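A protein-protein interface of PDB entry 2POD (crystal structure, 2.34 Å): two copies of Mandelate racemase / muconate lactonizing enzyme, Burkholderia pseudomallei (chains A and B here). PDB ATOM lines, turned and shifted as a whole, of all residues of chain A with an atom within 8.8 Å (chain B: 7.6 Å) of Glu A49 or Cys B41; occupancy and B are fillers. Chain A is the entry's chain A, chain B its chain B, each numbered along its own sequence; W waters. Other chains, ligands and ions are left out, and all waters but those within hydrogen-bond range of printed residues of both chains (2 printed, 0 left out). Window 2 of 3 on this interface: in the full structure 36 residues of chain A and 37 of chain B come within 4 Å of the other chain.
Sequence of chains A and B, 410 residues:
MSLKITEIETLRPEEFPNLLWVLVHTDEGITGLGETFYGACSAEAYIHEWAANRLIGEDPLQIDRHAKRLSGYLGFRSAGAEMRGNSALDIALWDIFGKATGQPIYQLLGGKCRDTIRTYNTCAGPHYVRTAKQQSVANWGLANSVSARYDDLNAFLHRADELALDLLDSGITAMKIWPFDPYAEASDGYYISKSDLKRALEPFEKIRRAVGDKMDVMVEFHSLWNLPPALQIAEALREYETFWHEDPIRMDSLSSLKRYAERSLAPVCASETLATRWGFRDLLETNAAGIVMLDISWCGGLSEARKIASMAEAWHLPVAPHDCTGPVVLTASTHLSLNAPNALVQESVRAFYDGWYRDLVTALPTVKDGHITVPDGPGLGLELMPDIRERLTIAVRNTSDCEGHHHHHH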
ATOM      1  N   THR A  10      10.478  17.776  -5.568  1.00  0.00           N
ATOM      2  CA  THR A  10       9.065  17.483  -5.814  1.00  0.00           C
ATOM      3  C   THR A  10       8.706  17.589  -7.289  1.00  0.00           C
ATOM      4  O   THR A  10       9.210  18.458  -8.000  1.00  0.00           O
ATOM      5  CB  THR A  10       8.136  18.405  -5.019  1.00  0.00           C
ATOM      6  OG1 THR A  10       8.468  19.764  -5.313  1.00  0.00           O
ATOM      7  CG2 THR A  10       8.261  18.140  -3.512  1.00  0.00           C
ATOM      8  N   CYS A  41      -0.104  21.388  -4.706  1.00  0.00           N
ATOM      9  CA  CYS A  41       0.648  22.633  -4.500  1.00  0.00           C
ATOM     10  C   CYS A  41       0.900  22.958  -3.042  1.00  0.00           C
ATOM     11  O   CYS A  41       1.976  23.432  -2.698  1.00  0.00           O
ATOM     12  CB  CYS A  41      -0.033  23.828  -5.169  1.00  0.00           C
ATOM     13  SG  CYS A  41      -0.185  23.695  -6.951  1.00  0.00           S
ATOM     14  N   SER A  42      -0.097  22.711  -2.194  1.00  0.00           N
ATOM     15  CA  SER A  42       0.018  23.013  -0.774  1.00  0.00           C
ATOM     16  C   SER A  42       0.907  22.021  -0.033  1.00  0.00           C
ATOM     17  O   SER A  42       1.645  22.407   0.876  1.00  0.00           O
ATOM     18  CB  SER A  42      -1.357  23.153  -0.107  1.00  0.00           C
ATOM     19  OG  SER A  42      -2.160  22.000  -0.283  1.00  0.00           O
ATOM     20  N   ALA A  43       0.843  20.750  -0.428  1.00  0.00           N
ATOM     21  CA  ALA A  43       1.799  19.756   0.051  1.00  0.00           C
ATOM     22  C   ALA A  43       3.233  20.092  -0.377  1.00  0.00           C
ATOM     23  O   ALA A  43       4.129  20.149   0.473  1.00  0.00           O
ATOM     24  CB  ALA A  43       1.402  18.360  -0.391  1.00  0.00           C
ATOM     25  N   GLU A  44       3.435  20.351  -1.675  1.00  0.00           N
ATOM     26  CA  GLU A  44       4.740  20.768  -2.213  1.00  0.00           C
ATOM     27  C   GLU A  44       5.298  22.011  -1.520  1.00  0.00           C
ATOM     28  O   GLU A  44       6.489  22.066  -1.194  1.00  0.00           O
ATOM     29  CB  GLU A  44       4.671  20.999  -3.730  1.00  0.00           C
ATOM     30  CG  GLU A  44       5.964  21.558  -4.333  1.00  0.00           C
ATOM     31  CD  GLU A  44       5.882  21.815  -5.826  1.00  0.00           C
ATOM     32  OE1 GLU A  44       6.455  21.016  -6.602  1.00  0.00           O
ATOM     33  OE2 GLU A  44       5.260  22.826  -6.223  1.00  0.00           O
ATOM     34  N   ALA A  45       4.433  22.995  -1.290  1.00  0.00           N
ATOM     35  CA  ALA A  45       4.847  24.241  -0.662  1.00  0.00           C
ATOM     36  C   ALA A  45       5.311  24.006   0.759  1.00  0.00           C
ATOM     37  O   ALA A  45       6.274  24.630   1.197  1.00  0.00           O
ATOM     38  CB  ALA A  45       3.736  25.261  -0.688  1.00  0.00           C
ATOM     39  N   TYR A  46       4.631  23.089   1.457  1.00  0.00           N
ATOM     40  CA  TYR A  46       4.968  22.735   2.830  1.00  0.00           C
ATOM     41  C   TYR A  46       6.330  22.059   2.901  1.00  0.00           C
ATOM     42  O   TYR A  46       7.148  22.409   3.760  1.00  0.00           O
ATOM     43  CB  TYR A  46       3.888  21.842   3.470  1.00  0.00           C
ATOM     44  CG  TYR A  46       4.413  21.007   4.625  1.00  0.00           C
ATOM     45  CD1 TYR A  46       4.711  19.652   4.454  1.00  0.00           C
ATOM     46  CD2 TYR A  46       4.656  21.587   5.875  1.00  0.00           C
ATOM     47  CE1 TYR A  46       5.216  18.897   5.500  1.00  0.00           C
ATOM     48  CE2 TYR A  46       5.156  20.836   6.930  1.00  0.00           C
ATOM     49  CZ  TYR A  46       5.430  19.493   6.737  1.00  0.00           C
ATOM     50  OH  TYR A  46       5.926  18.747   7.777  1.00  0.00           O
ATOM     51  N   ILE A  47       6.565  21.085   2.021  1.00  0.00           N
ATOM     52  CA  ILE A  47       7.832  20.361   2.064  1.00  0.00           C
ATOM     53  C   ILE A  47       9.068  21.219   1.829  1.00  0.00           C
ATOM     54  O   ILE A  47      10.063  21.068   2.530  1.00  0.00           O
ATOM     55  CB  ILE A  47       7.854  18.962   1.370  1.00  0.00           C
ATOM     56  CG1 ILE A  47       7.071  18.920   0.069  1.00  0.00           C
ATOM     57  CG2 ILE A  47       7.201  17.943   2.256  1.00  0.00           C
ATOM     58  CD1 ILE A  47       6.459  17.521  -0.212  1.00  0.00           C
ATOM     59  N   HIS A  48       8.969  22.172   0.909  1.00  0.00           N
ATOM     60  CA  HIS A  48      10.024  23.164   0.729  1.00  0.00           C
ATOM     61  C   HIS A  48      10.084  24.272   1.774  1.00  0.00           C
ATOM     62  O   HIS A  48      11.168  24.777   2.071  1.00  0.00           O
ATOM     63  CB  HIS A  48       9.986  23.742  -0.678  1.00  0.00           C
ATOM     64  CG  HIS A  48      10.207  22.711  -1.731  1.00  0.00           C
ATOM     65  ND1 HIS A  48       9.190  22.228  -2.522  1.00  0.00           N
ATOM     66  CD2 HIS A  48      11.323  22.039  -2.096  1.00  0.00           C
ATOM     67  CE1 HIS A  48       9.675  21.312  -3.341  1.00  0.00           C
ATOM     68  NE2 HIS A  48      10.965  21.176  -3.101  1.00  0.00           N
ATOM     69  N   GLU A  49       8.936  24.651   2.332  1.00  0.00           N
ATOM     70  CA  GLU A  49       8.919  25.720   3.327  1.00  0.00           C
ATOM     71  C   GLU A  49       9.459  25.273   4.687  1.00  0.00           C
ATOM     72  O   GLU A  49      10.154  26.036   5.365  1.00  0.00           O
ATOM     73  CB  GLU A  49       7.531  26.356   3.450  1.00  0.00           C
ATOM     74  CG  GLU A  49       7.499  27.634   4.281  1.00  0.00           C
ATOM     75  CD  GLU A  49       6.094  28.157   4.529  1.00  0.00           C
ATOM     76  OE1 GLU A  49       5.959  29.357   4.861  1.00  0.00           O
ATOM     77  OE2 GLU A  49       5.125  27.379   4.383  1.00  0.00           O
ATOM     78  N   TRP A  50       9.151  24.037   5.072  1.00  0.00           N
ATOM     79  CA  TRP A  50       9.441  23.566   6.420  1.00  0.00           C
ATOM     80  C   TRP A  50      10.173  22.226   6.467  1.00  0.00           C
ATOM     81  O   TRP A  50      11.174  22.087   7.174  1.00  0.00           O
ATOM     82  CB  TRP A  50       8.156  23.491   7.242  1.00  0.00           C
ATOM     83  CG  TRP A  50       8.378  23.350   8.722  1.00  0.00           C
ATOM     84  CD1 TRP A  50       8.715  24.340   9.602  1.00  0.00           C
ATOM     85  CD2 TRP A  50       8.269  22.149   9.494  1.00  0.00           C
ATOM     86  NE1 TRP A  50       8.824  23.828  10.874  1.00  0.00           N
ATOM     87  CE2 TRP A  50       8.552  22.487  10.836  1.00  0.00           C
ATOM     88  CE3 TRP A  50       7.961  20.819   9.182  1.00  0.00           C
ATOM     89  CZ2 TRP A  50       8.525  21.541  11.869  1.00  0.00           C
ATOM     90  CZ3 TRP A  50       7.934  19.881  10.205  1.00  0.00           C
ATOM     91  CH2 TRP A  50       8.214  20.246  11.533  1.00  0.00           C
ATOM     92  N   ALA A  51       9.660  21.239   5.738  1.00  0.00           N
ATOM     93  CA  ALA A  51      10.008  19.844   5.996  1.00  0.00           C
ATOM     94  C   ALA A  51      11.401  19.480   5.489  1.00  0.00           C
ATOM     95  O   ALA A  51      12.164  18.831   6.196  1.00  0.00           O
ATOM     96  CB  ALA A  51       8.957  18.905   5.419  1.00  0.00           C
ATOM     97  N   ALA A  52      11.730  19.928   4.281  1.00  0.00           N
ATOM     98  CA  ALA A  52      13.038  19.689   3.669  1.00  0.00           C
ATOM     99  C   ALA A  52      14.232  20.128   4.508  1.00  0.00           C
ATOM    100  O   ALA A  52      15.241  19.424   4.559  1.00  0.00           O
ATOM    101  CB  ALA A  52      13.103  20.331   2.334  1.00  0.00           C
ATOM    102  N   ASN A  53      14.112  21.276   5.172  1.00  0.00           N
ATOM    103  CA  ASN A  53      15.198  21.809   5.992  1.00  0.00           C
ATOM    104  C   ASN A  53      15.407  21.054   7.300  1.00  0.00           C
ATOM    105  O   ASN A  53      16.446  21.185   7.956  1.00  0.00           O
ATOM    106  CB  ASN A  53      15.010  23.304   6.238  1.00  0.00           C
ATOM    107  CG  ASN A  53      15.191  24.123   4.973  1.00  0.00           C
ATOM    108  OD1 ASN A  53      16.180  23.963   4.257  1.00  0.00           O
ATOM    109  ND2 ASN A  53      14.226  24.996   4.682  1.00  0.00           N
ATOM    110  N   ARG A  54      14.422  20.246   7.663  1.00  0.00           N
ATOM    111  CA  ARG A  54      14.527  19.416   8.848  1.00  0.00           C
ATOM    112  C   ARG A  54      15.084  18.033   8.562  1.00  0.00           C
ATOM    113  O   ARG A  54      15.448  17.312   9.485  1.00  0.00           O
ATOM    114  CB  ARG A  54      13.186  19.338   9.570  1.00  0.00           C
ATOM    115  CG  ARG A  54      12.932  20.559  10.413  1.00  0.00           C
ATOM    116  CD  ARG A  54      11.698  20.396  11.235  1.00  0.00           C
ATOM    117  NE  ARG A  54      11.926  19.637  12.462  1.00  0.00           N
ATOM    118  CZ  ARG A  54      12.100  20.178  13.664  1.00  0.00           C
ATOM    119  NH1 ARG A  54      12.294  19.395  14.718  1.00  0.00           N
ATOM    120  NH2 ARG A  54      12.079  21.498  13.819  1.00  0.00           N
ATOM    121  N   ALA A  81      -2.229  19.424   4.468  1.00  0.00           N
ATOM    122  CA  ALA A  81      -1.104  19.493   3.524  1.00  0.00           C
ATOM    123  C   ALA A  81       0.224  19.105   4.162  1.00  0.00           C
ATOM    124  O   ALA A  81       0.992  18.345   3.586  1.00  0.00           O
ATOM    125  CB  ALA A  81      -1.012  20.876   2.908  1.00  0.00           C
ATOM    126  N   GLU A  82       0.466  19.624   5.361  1.00  0.00           N
ATOM    127  CA  GLU A  82       1.526  19.154   6.250  1.00  0.00           C
ATOM    128  C   GLU A  82       1.566  17.629   6.392  1.00  0.00           C
ATOM    129  O   GLU A  82       2.627  17.023   6.252  1.00  0.00           O
ATOM    130  CB  GLU A  82       1.387  19.812   7.636  1.00  0.00           C
ATOM    131  CG  GLU A  82       1.481  21.349   7.634  1.00  0.00           C
ATOM    132  CD  GLU A  82       0.145  22.075   7.425  1.00  0.00           C
ATOM    133  OE1 GLU A  82      -0.828  21.481   6.907  1.00  0.00           O
ATOM    134  OE2 GLU A  82       0.077  23.269   7.773  1.00  0.00           O
ATOM    135  N   ARG A 397      10.632  21.140  -8.501  1.00  0.00           N
ATOM    136  CA  ARG A 397      11.085  22.089  -7.500  1.00  0.00           C
ATOM    137  C   ARG A 397      12.135  21.406  -6.629  1.00  0.00           C
ATOM    138  O   ARG A 397      12.062  20.200  -6.390  1.00  0.00           O
ATOM    139  CB  ARG A 397       9.892  22.564  -6.677  1.00  0.00           C
ATOM    140  CG  ARG A 397      10.152  23.790  -5.835  1.00  0.00           C
ATOM    141  CD  ARG A 397       9.043  24.830  -5.979  1.00  0.00           C
ATOM    142  NE  ARG A 397       8.624  25.396  -4.696  1.00  0.00           N
ATOM    143  CZ  ARG A 397       9.382  26.153  -3.902  1.00  0.00           C
ATOM    144  NH1 ARG A 397       8.884  26.615  -2.767  1.00  0.00           N
ATOM    145  NH2 ARG A 397      10.635  26.461  -4.227  1.00  0.00           N
ATOM    146  N   THR A 399      15.282  21.630  -3.404  1.00  0.00           N
ATOM    147  CA  THR A 399      15.821  22.197  -2.161  1.00  0.00           C
ATOM    148  C   THR A 399      17.124  21.527  -1.719  1.00  0.00           C
ATOM    149  O   THR A 399      17.277  20.310  -1.819  1.00  0.00           O
ATOM    150  CB  THR A 399      14.784  22.147  -1.012  1.00  0.00           C
ATOM    151  OG1 THR A 399      15.390  22.553   0.225  1.00  0.00           O
ATOM    152  CG2 THR A 399      14.230  20.750  -0.863  1.00  0.00           C
ATOM    153  N   ARG B  12       2.945  37.855   1.015  1.00  0.00           N
ATOM    154  CA  ARG B  12       3.932  37.236   1.898  1.00  0.00           C
ATOM    155  C   ARG B  12       5.156  38.130   2.120  1.00  0.00           C
ATOM    156  O   ARG B  12       6.053  38.180   1.275  1.00  0.00           O
ATOM    157  CB  ARG B  12       4.381  35.887   1.339  1.00  0.00           C
ATOM    158  CG  ARG B  12       3.370  34.765   1.468  1.00  0.00           C
ATOM    159  CD  ARG B  12       4.027  33.396   1.285  1.00  0.00           C
ATOM    160  NE  ARG B  12       4.438  33.157  -0.098  1.00  0.00           N
ATOM    161  CZ  ARG B  12       5.694  33.220  -0.537  1.00  0.00           C
ATOM    162  NH1 ARG B  12       5.961  32.990  -1.814  1.00  0.00           N
ATOM    163  NH2 ARG B  12       6.683  33.512   0.296  1.00  0.00           N
ATOM    164  N   PRO B  17       8.263  35.976   7.730  1.00  0.00           N
ATOM    165  CA  PRO B  17       7.968  34.880   6.800  1.00  0.00           C
ATOM    166  C   PRO B  17       6.882  33.892   7.266  1.00  0.00           C
ATOM    167  O   PRO B  17       6.391  33.103   6.459  1.00  0.00           O
ATOM    168  CB  PRO B  17       9.324  34.181   6.633  1.00  0.00           C
ATOM    169  CG  PRO B  17      10.068  34.483   7.891  1.00  0.00           C
ATOM    170  CD  PRO B  17       9.584  35.821   8.374  1.00  0.00           C
ATOM    171  N   ASN B  18       6.497  33.946   8.538  1.00  0.00           N
ATOM    172  CA  ASN B  18       5.347  33.167   9.013  1.00  0.00           C
ATOM    173  C   ASN B  18       3.992  33.793   8.672  1.00  0.00           C
ATOM    174  O   ASN B  18       2.958  33.120   8.722  1.00  0.00           O
ATOM    175  CB  ASN B  18       5.439  32.916  10.517  1.00  0.00           C
ATOM    176  CG  ASN B  18       6.493  31.896  10.879  1.00  0.00           C
ATOM    177  OD1 ASN B  18       7.210  32.063  11.866  1.00  0.00           O
ATOM    178  ND2 ASN B  18       6.583  30.822  10.098  1.00  0.00           N
ATOM    179  N   LEU B  19       4.012  35.076   8.319  1.00  0.00           N
ATOM    180  CA  LEU B  19       2.808  35.882   8.189  1.00  0.00           C
ATOM    181  C   LEU B  19       2.220  35.792   6.791  1.00  0.00           C
ATOM    182  O   LEU B  19       2.943  35.824   5.795  1.00  0.00           O
ATOM    183  CB  LEU B  19       3.120  37.336   8.542  1.00  0.00           C
ATOM    184  CG  LEU B  19       2.051  38.424   8.646  1.00  0.00           C
ATOM    185  CD1 LEU B  19       1.066  38.158   9.772  1.00  0.00           C
ATOM    186  CD2 LEU B  19       2.772  39.728   8.893  1.00  0.00           C
ATOM    187  N   LEU B  20       0.898  35.676   6.719  1.00  0.00           N
ATOM    188  CA  LEU B  20       0.212  35.755   5.443  1.00  0.00           C
ATOM    189  C   LEU B  20      -0.964  36.717   5.529  1.00  0.00           C
ATOM    190  O   LEU B  20      -1.822  36.566   6.390  1.00  0.00           O
ATOM    191  CB  LEU B  20      -0.232  34.366   4.978  1.00  0.00           C
ATOM    192  CG  LEU B  20      -1.081  34.253   3.709  1.00  0.00           C
ATOM    193  CD1 LEU B  20      -0.261  34.595   2.477  1.00  0.00           C
ATOM    194  CD2 LEU B  20      -1.656  32.850   3.579  1.00  0.00           C
ATOM    195  N   TYR B  38       2.015  31.137  10.635  1.00  0.00           N
ATOM    196  CA  TYR B  38       2.675  29.860  10.323  1.00  0.00           C
ATOM    197  C   TYR B  38       2.338  29.268   8.969  1.00  0.00           C
ATOM    198  O   TYR B  38       1.214  29.400   8.495  1.00  0.00           O
ATOM    199  CB  TYR B  38       2.523  28.804  11.434  1.00  0.00           C
ATOM    200  CG  TYR B  38       3.066  29.225  12.778  1.00  0.00           C
ATOM    201  CD1 TYR B  38       4.309  29.854  12.895  1.00  0.00           C
ATOM    202  CD2 TYR B  38       2.339  28.987  13.938  1.00  0.00           C
ATOM    203  CE1 TYR B  38       4.805  30.239  14.139  1.00  0.00           C
ATOM    204  CE2 TYR B  38       2.821  29.371  15.184  1.00  0.00           C
ATOM    205  CZ  TYR B  38       4.052  29.997  15.278  1.00  0.00           C
ATOM    206  OH  TYR B  38       4.519  30.367  16.518  1.00  0.00           O
ATOM    207  N   GLY B  39       3.332  28.613   8.358  1.00  0.00           N
ATOM    208  CA  GLY B  39       3.167  27.863   7.111  1.00  0.00           C
ATOM    209  C   GLY B  39       2.542  28.677   5.997  1.00  0.00           C
ATOM    210  O   GLY B  39       1.636  28.196   5.302  1.00  0.00           O
ATOM    211  N   ALA B  40       3.026  29.914   5.842  1.00  0.00           N
ATOM    212  CA  ALA B  40       2.459  30.889   4.911  1.00  0.00           C
ATOM    213  C   ALA B  40       2.407  30.407   3.470  1.00  0.00           C
ATOM    214  O   ALA B  40       1.394  30.601   2.800  1.00  0.00           O
ATOM    215  CB  ALA B  40       3.192  32.224   5.003  1.00  0.00           C
ATOM    216  N   CYS B  41       3.487  29.780   3.003  1.00  0.00           N
ATOM    217  CA  CYS B  41       3.556  29.264   1.630  1.00  0.00           C
ATOM    218  C   CYS B  41       2.564  28.150   1.349  1.00  0.00           C
ATOM    219  O   CYS B  41       2.073  28.042   0.234  1.00  0.00           O
ATOM    220  CB  CYS B  41       4.960  28.769   1.285  1.00  0.00           C
ATOM    221  SG  CYS B  41       6.178  30.067   1.175  1.00  0.00           S
ATOM    222  N   SER B  42       2.285  27.318   2.351  1.00  0.00           N
ATOM    223  CA  SER B  42       1.366  26.201   2.165  1.00  0.00           C
ATOM    224  C   SER B  42      -0.090  26.651   2.205  1.00  0.00           C
ATOM    225  O   SER B  42      -0.911  26.180   1.410  1.00  0.00           O
ATOM    226  CB  SER B  42       1.645  25.063   3.151  1.00  0.00           C
ATOM    227  OG  SER B  42       1.476  25.469   4.496  1.00  0.00           O
ATOM    228  N   ALA B  43      -0.395  27.577   3.114  1.00  0.00           N
ATOM    229  CA  ALA B  43      -1.697  28.241   3.139  1.00  0.00           C
ATOM    230  C   ALA B  43      -1.977  29.061   1.875  1.00  0.00           C
ATOM    231  O   ALA B  43      -3.082  28.986   1.323  1.00  0.00           O
ATOM    232  CB  ALA B  43      -1.848  29.092   4.396  1.00  0.00           C
ATOM    233  N   GLU B  44      -0.978  29.814   1.407  1.00  0.00           N
ATOM    234  CA  GLU B  44      -1.082  30.563   0.148  1.00  0.00           C
ATOM    235  C   GLU B  44      -1.321  29.636  -1.045  1.00  0.00           C
ATOM    236  O   GLU B  44      -2.202  29.887  -1.871  1.00  0.00           O
ATOM    237  CB  GLU B  44       0.165  31.435  -0.085  1.00  0.00           C
ATOM    238  CG  GLU B  44       0.274  32.024  -1.492  1.00  0.00           C
ATOM    239  CD  GLU B  44       1.515  32.870  -1.697  1.00  0.00           C
ATOM    240  OE1 GLU B  44       1.395  34.118  -1.672  1.00  0.00           O
ATOM    241  OE2 GLU B  44       2.604  32.287  -1.894  1.00  0.00           O
ATOM    242  N   ALA B  45      -0.547  28.559  -1.117  1.00  0.00           N
ATOM    243  CA  ALA B  45      -0.656  27.617  -2.221  1.00  0.00           C
ATOM    244  C   ALA B  45      -2.027  26.954  -2.267  1.00  0.00           C
ATOM    245  O   ALA B  45      -2.572  26.749  -3.351  1.00  0.00           O
ATOM    246  CB  ALA B  45       0.447  26.580  -2.157  1.00  0.00           C
ATOM    247  N   TYR B  46      -2.579  26.647  -1.089  1.00  0.00           N
ATOM    248  CA  TYR B  46      -3.943  26.128  -0.958  1.00  0.00           C
ATOM    249  C   TYR B  46      -5.002  27.115  -1.471  1.00  0.00           C
ATOM    250  O   TYR B  46      -5.924  26.719  -2.190  1.00  0.00           O
ATOM    251  CB  TYR B  46      -4.252  25.740   0.501  1.00  0.00           C
ATOM    252  CG  TYR B  46      -5.740  25.660   0.784  1.00  0.00           C
ATOM    253  CD1 TYR B  46      -6.401  26.690   1.463  1.00  0.00           C
ATOM    254  CD2 TYR B  46      -6.496  24.576   0.325  1.00  0.00           C
ATOM    255  CE1 TYR B  46      -7.762  26.630   1.689  1.00  0.00           C
ATOM    256  CE2 TYR B  46      -7.857  24.510   0.553  1.00  0.00           C
ATOM    257  CZ  TYR B  46      -8.483  25.533   1.236  1.00  0.00           C
ATOM    258  OH  TYR B  46      -9.835  25.464   1.453  1.00  0.00           O
ATOM    259  N   ILE B  47      -4.886  28.381  -1.067  1.00  0.00           N
ATOM    260  CA  ILE B  47      -5.830  29.419  -1.495  1.00  0.00           C
ATOM    261  C   ILE B  47      -5.934  29.506  -3.019  1.00  0.00           C
ATOM    262  O   ILE B  47      -7.034  29.455  -3.564  1.00  0.00           O
ATOM    263  CB  ILE B  47      -5.516  30.784  -0.870  1.00  0.00           C
ATOM    264  CG1 ILE B  47      -5.899  30.776   0.614  1.00  0.00           C
ATOM    265  CG2 ILE B  47      -6.252  31.926  -1.615  1.00  0.00           C
ATOM    266  CD1 ILE B  47      -5.414  32.003   1.387  1.00  0.00           C
ATOM    267  N   HIS B  48      -4.788  29.565  -3.693  1.00  0.00           N
ATOM    268  CA  HIS B  48      -4.748  29.702  -5.143  1.00  0.00           C
ATOM    269  C   HIS B  48      -5.052  28.393  -5.882  1.00  0.00           C
ATOM    270  O   HIS B  48      -5.567  28.420  -7.006  1.00  0.00           O
ATOM    271  CB  HIS B  48      -3.415  30.322  -5.600  1.00  0.00           C
ATOM    272  CG  HIS B  48      -3.166  31.691  -5.043  1.00  0.00           C
ATOM    273  ND1 HIS B  48      -3.917  32.789  -5.404  1.00  0.00           N
ATOM    274  CD2 HIS B  48      -2.255  32.141  -4.146  1.00  0.00           C
ATOM    275  CE1 HIS B  48      -3.481  33.854  -4.756  1.00  0.00           C
ATOM    276  NE2 HIS B  48      -2.473  33.489  -3.985  1.00  0.00           N
ATOM    277  N   ALA B  81      -2.879  23.588   6.560  1.00  0.00           N
ATOM    278  CA  ALA B  81      -2.781  24.677   5.569  1.00  0.00           C
ATOM    279  C   ALA B  81      -4.142  25.086   5.017  1.00  0.00           C
ATOM    280  O   ALA B  81      -4.461  26.272   4.948  1.00  0.00           O
ATOM    281  CB  ALA B  81      -1.845  24.297   4.434  1.00  0.00           C
ATOM    282  N   ARG B  84      -6.055  27.068   7.854  1.00  0.00           N
ATOM    283  CA  ARG B  84      -5.532  28.424   8.028  1.00  0.00           C
ATOM    284  C   ARG B  84      -5.876  29.325   6.835  1.00  0.00           C
ATOM    285  O   ARG B  84      -6.158  30.510   7.003  1.00  0.00           O
ATOM    286  CB  ARG B  84      -4.020  28.392   8.262  1.00  0.00           C
ATOM    287  CG  ARG B  84      -3.591  27.695   9.553  1.00  0.00           C
ATOM    288  CD  ARG B  84      -2.095  27.906   9.853  1.00  0.00           C
ATOM    289  NE  ARG B  84      -1.242  27.687   8.686  1.00  0.00           N
ATOM    290  CZ  ARG B  84      -0.761  26.508   8.297  1.00  0.00           C
ATOM    291  NH1 ARG B  84      -0.005  26.436   7.215  1.00  0.00           N
ATOM    292  NH2 ARG B  84      -1.032  25.400   8.977  1.00  0.00           N
ATOM    293  N   ARG B 397       0.799  37.161  -4.911  1.00  0.00           N
ATOM    294  CA  ARG B 397       0.197  36.242  -5.863  1.00  0.00           C
ATOM    295  C   ARG B 397      -1.282  36.597  -5.999  1.00  0.00           C
ATOM    296  O   ARG B 397      -1.899  37.091  -5.055  1.00  0.00           O
ATOM    297  CB  ARG B 397       0.400  34.789  -5.408  1.00  0.00           C
ATOM    298  CG  ARG B 397       0.112  33.731  -6.477  1.00  0.00           C
ATOM    299  CD  ARG B 397       1.311  32.823  -6.726  1.00  0.00           C
ATOM    300  NE  ARG B 397       1.334  31.656  -5.845  1.00  0.00           N
ATOM    301  CZ  ARG B 397       0.706  30.505  -6.086  1.00  0.00           C
ATOM    302  NH1 ARG B 397       0.805  29.511  -5.215  1.00  0.00           N
ATOM    303  NH2 ARG B 397      -0.022  30.341  -7.184  1.00  0.00           N
HETATM  304  O   HOH W   1       4.242  24.975   5.317  1.00  0.00           O
HETATM  305  O   HOH W   2       8.268  30.791   4.142  1.00  0.00           O
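The backbone NH (N) of Ala B40 sits at hydrogen-bond distance from the side-chain carboxylate (OE1) of Glu A49, 3.1 Å away. N of Cys B41 sits at hydrogen-bond distance from OE1 of Glu A49, at 3.1 Å. The side-chain carboxylate of Glu A49 lies within hydrogen-bond range of the backbone NH of Ser B42 (3.5 Å). N of Ala B81 is in hydrogen-bond range of OE1 of Glu A82, at 3.0 Å. NH2 of Arg B84 lies within salt-bridge range of OE2 of Glu A82 (2.7 Å).
Ser B42 touches its own counterpart, Ser A42. Ser A42 touches Ala B45, and with the chains exchanged Ala A45 touches Ser B42. Ala B81 touches its own counterpart, Ala A81.
Of the 19 printed residues of chain B, 8 touch a printed residue of chain A. Hydrophobic or aromatic side chains of chain B within 4 Å of the printed part of chain A: Ala B40, Ala B45, Tyr B46 and Ala B81. Among the printed residues, Asp or Glu carboxylates within 4 Å of a Lys or Arg side-chain nitrogen of the other chain: Glu A82 with Arg B84.
Water W1 bridges the side-chain carboxylate of Glu A49 (2.7 Å) and the side-chain hydroxyl of Ser B42 (2.9 Å). Water W2 lies within hydrogen-bond range of the side-chain carboxylate of Glu A49 and the side-chain sulfur of Cys B41.
Among the printed residues, merely in contact across the chains: Glu A49 with Gly B39 (3.3 Å), Ala A45 with Cys B41 (3.4 Å), Ser A42 with Ser B42 (3.4 Å), Cys A41 with Ala B45 (3.5 Å), Ala A45 with Ser B42 (3.8 Å), Ser A42 with Tyr B46 (3.8 Å), Ala A45 with Ala B45 (3.8 Å), Ala A81 with Ala B81 (3.8 Å), Ser A42 with Ala B45 (3.8 Å) and Tyr A46 with Ser B42 (3.9 Å).
Of the printed residues of chain B, Ser A42 touches Ser B42 (3.4 Å), Ala B45 (3.8 Å) and Tyr B46 (3.8 Å). Printed residues of chain B within 4 Å of Glu A49: Gly B39 (3.3 Å), Ala B40 (3.1 Å), Cys B41 (3.1 Å) and Ser B42 (3.5 Å). Gly B39 touches one residue of chain A. Ala B40 touches one residue of chain A. Cys B41 touches just these residues of chain A: Ala A45 and Glu A49. Of chain A, only Ser A42, Ala A45, Tyr A46 and Glu A49 come within 4 Å of Ser B42. The nearest residue of chain B that does not touch Glu A49 is Pro B17 (4.1 Å). The nearest printed residue of chain A that does not touch Cys B41 is Cys A41 (5.5 Å).
NE of Arg B84 lies within hydrogen-bond range of O of Tyr B38, 3.0 Å away. The side-chain hydroxyl (OG) of Ser B42 is in hydrogen-bond range of the backbone carbonyl oxygen (O) of Gly B39, 2.8 Å away. NH1 of Arg B84 lies within hydrogen-bond range of O of Gly B39.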
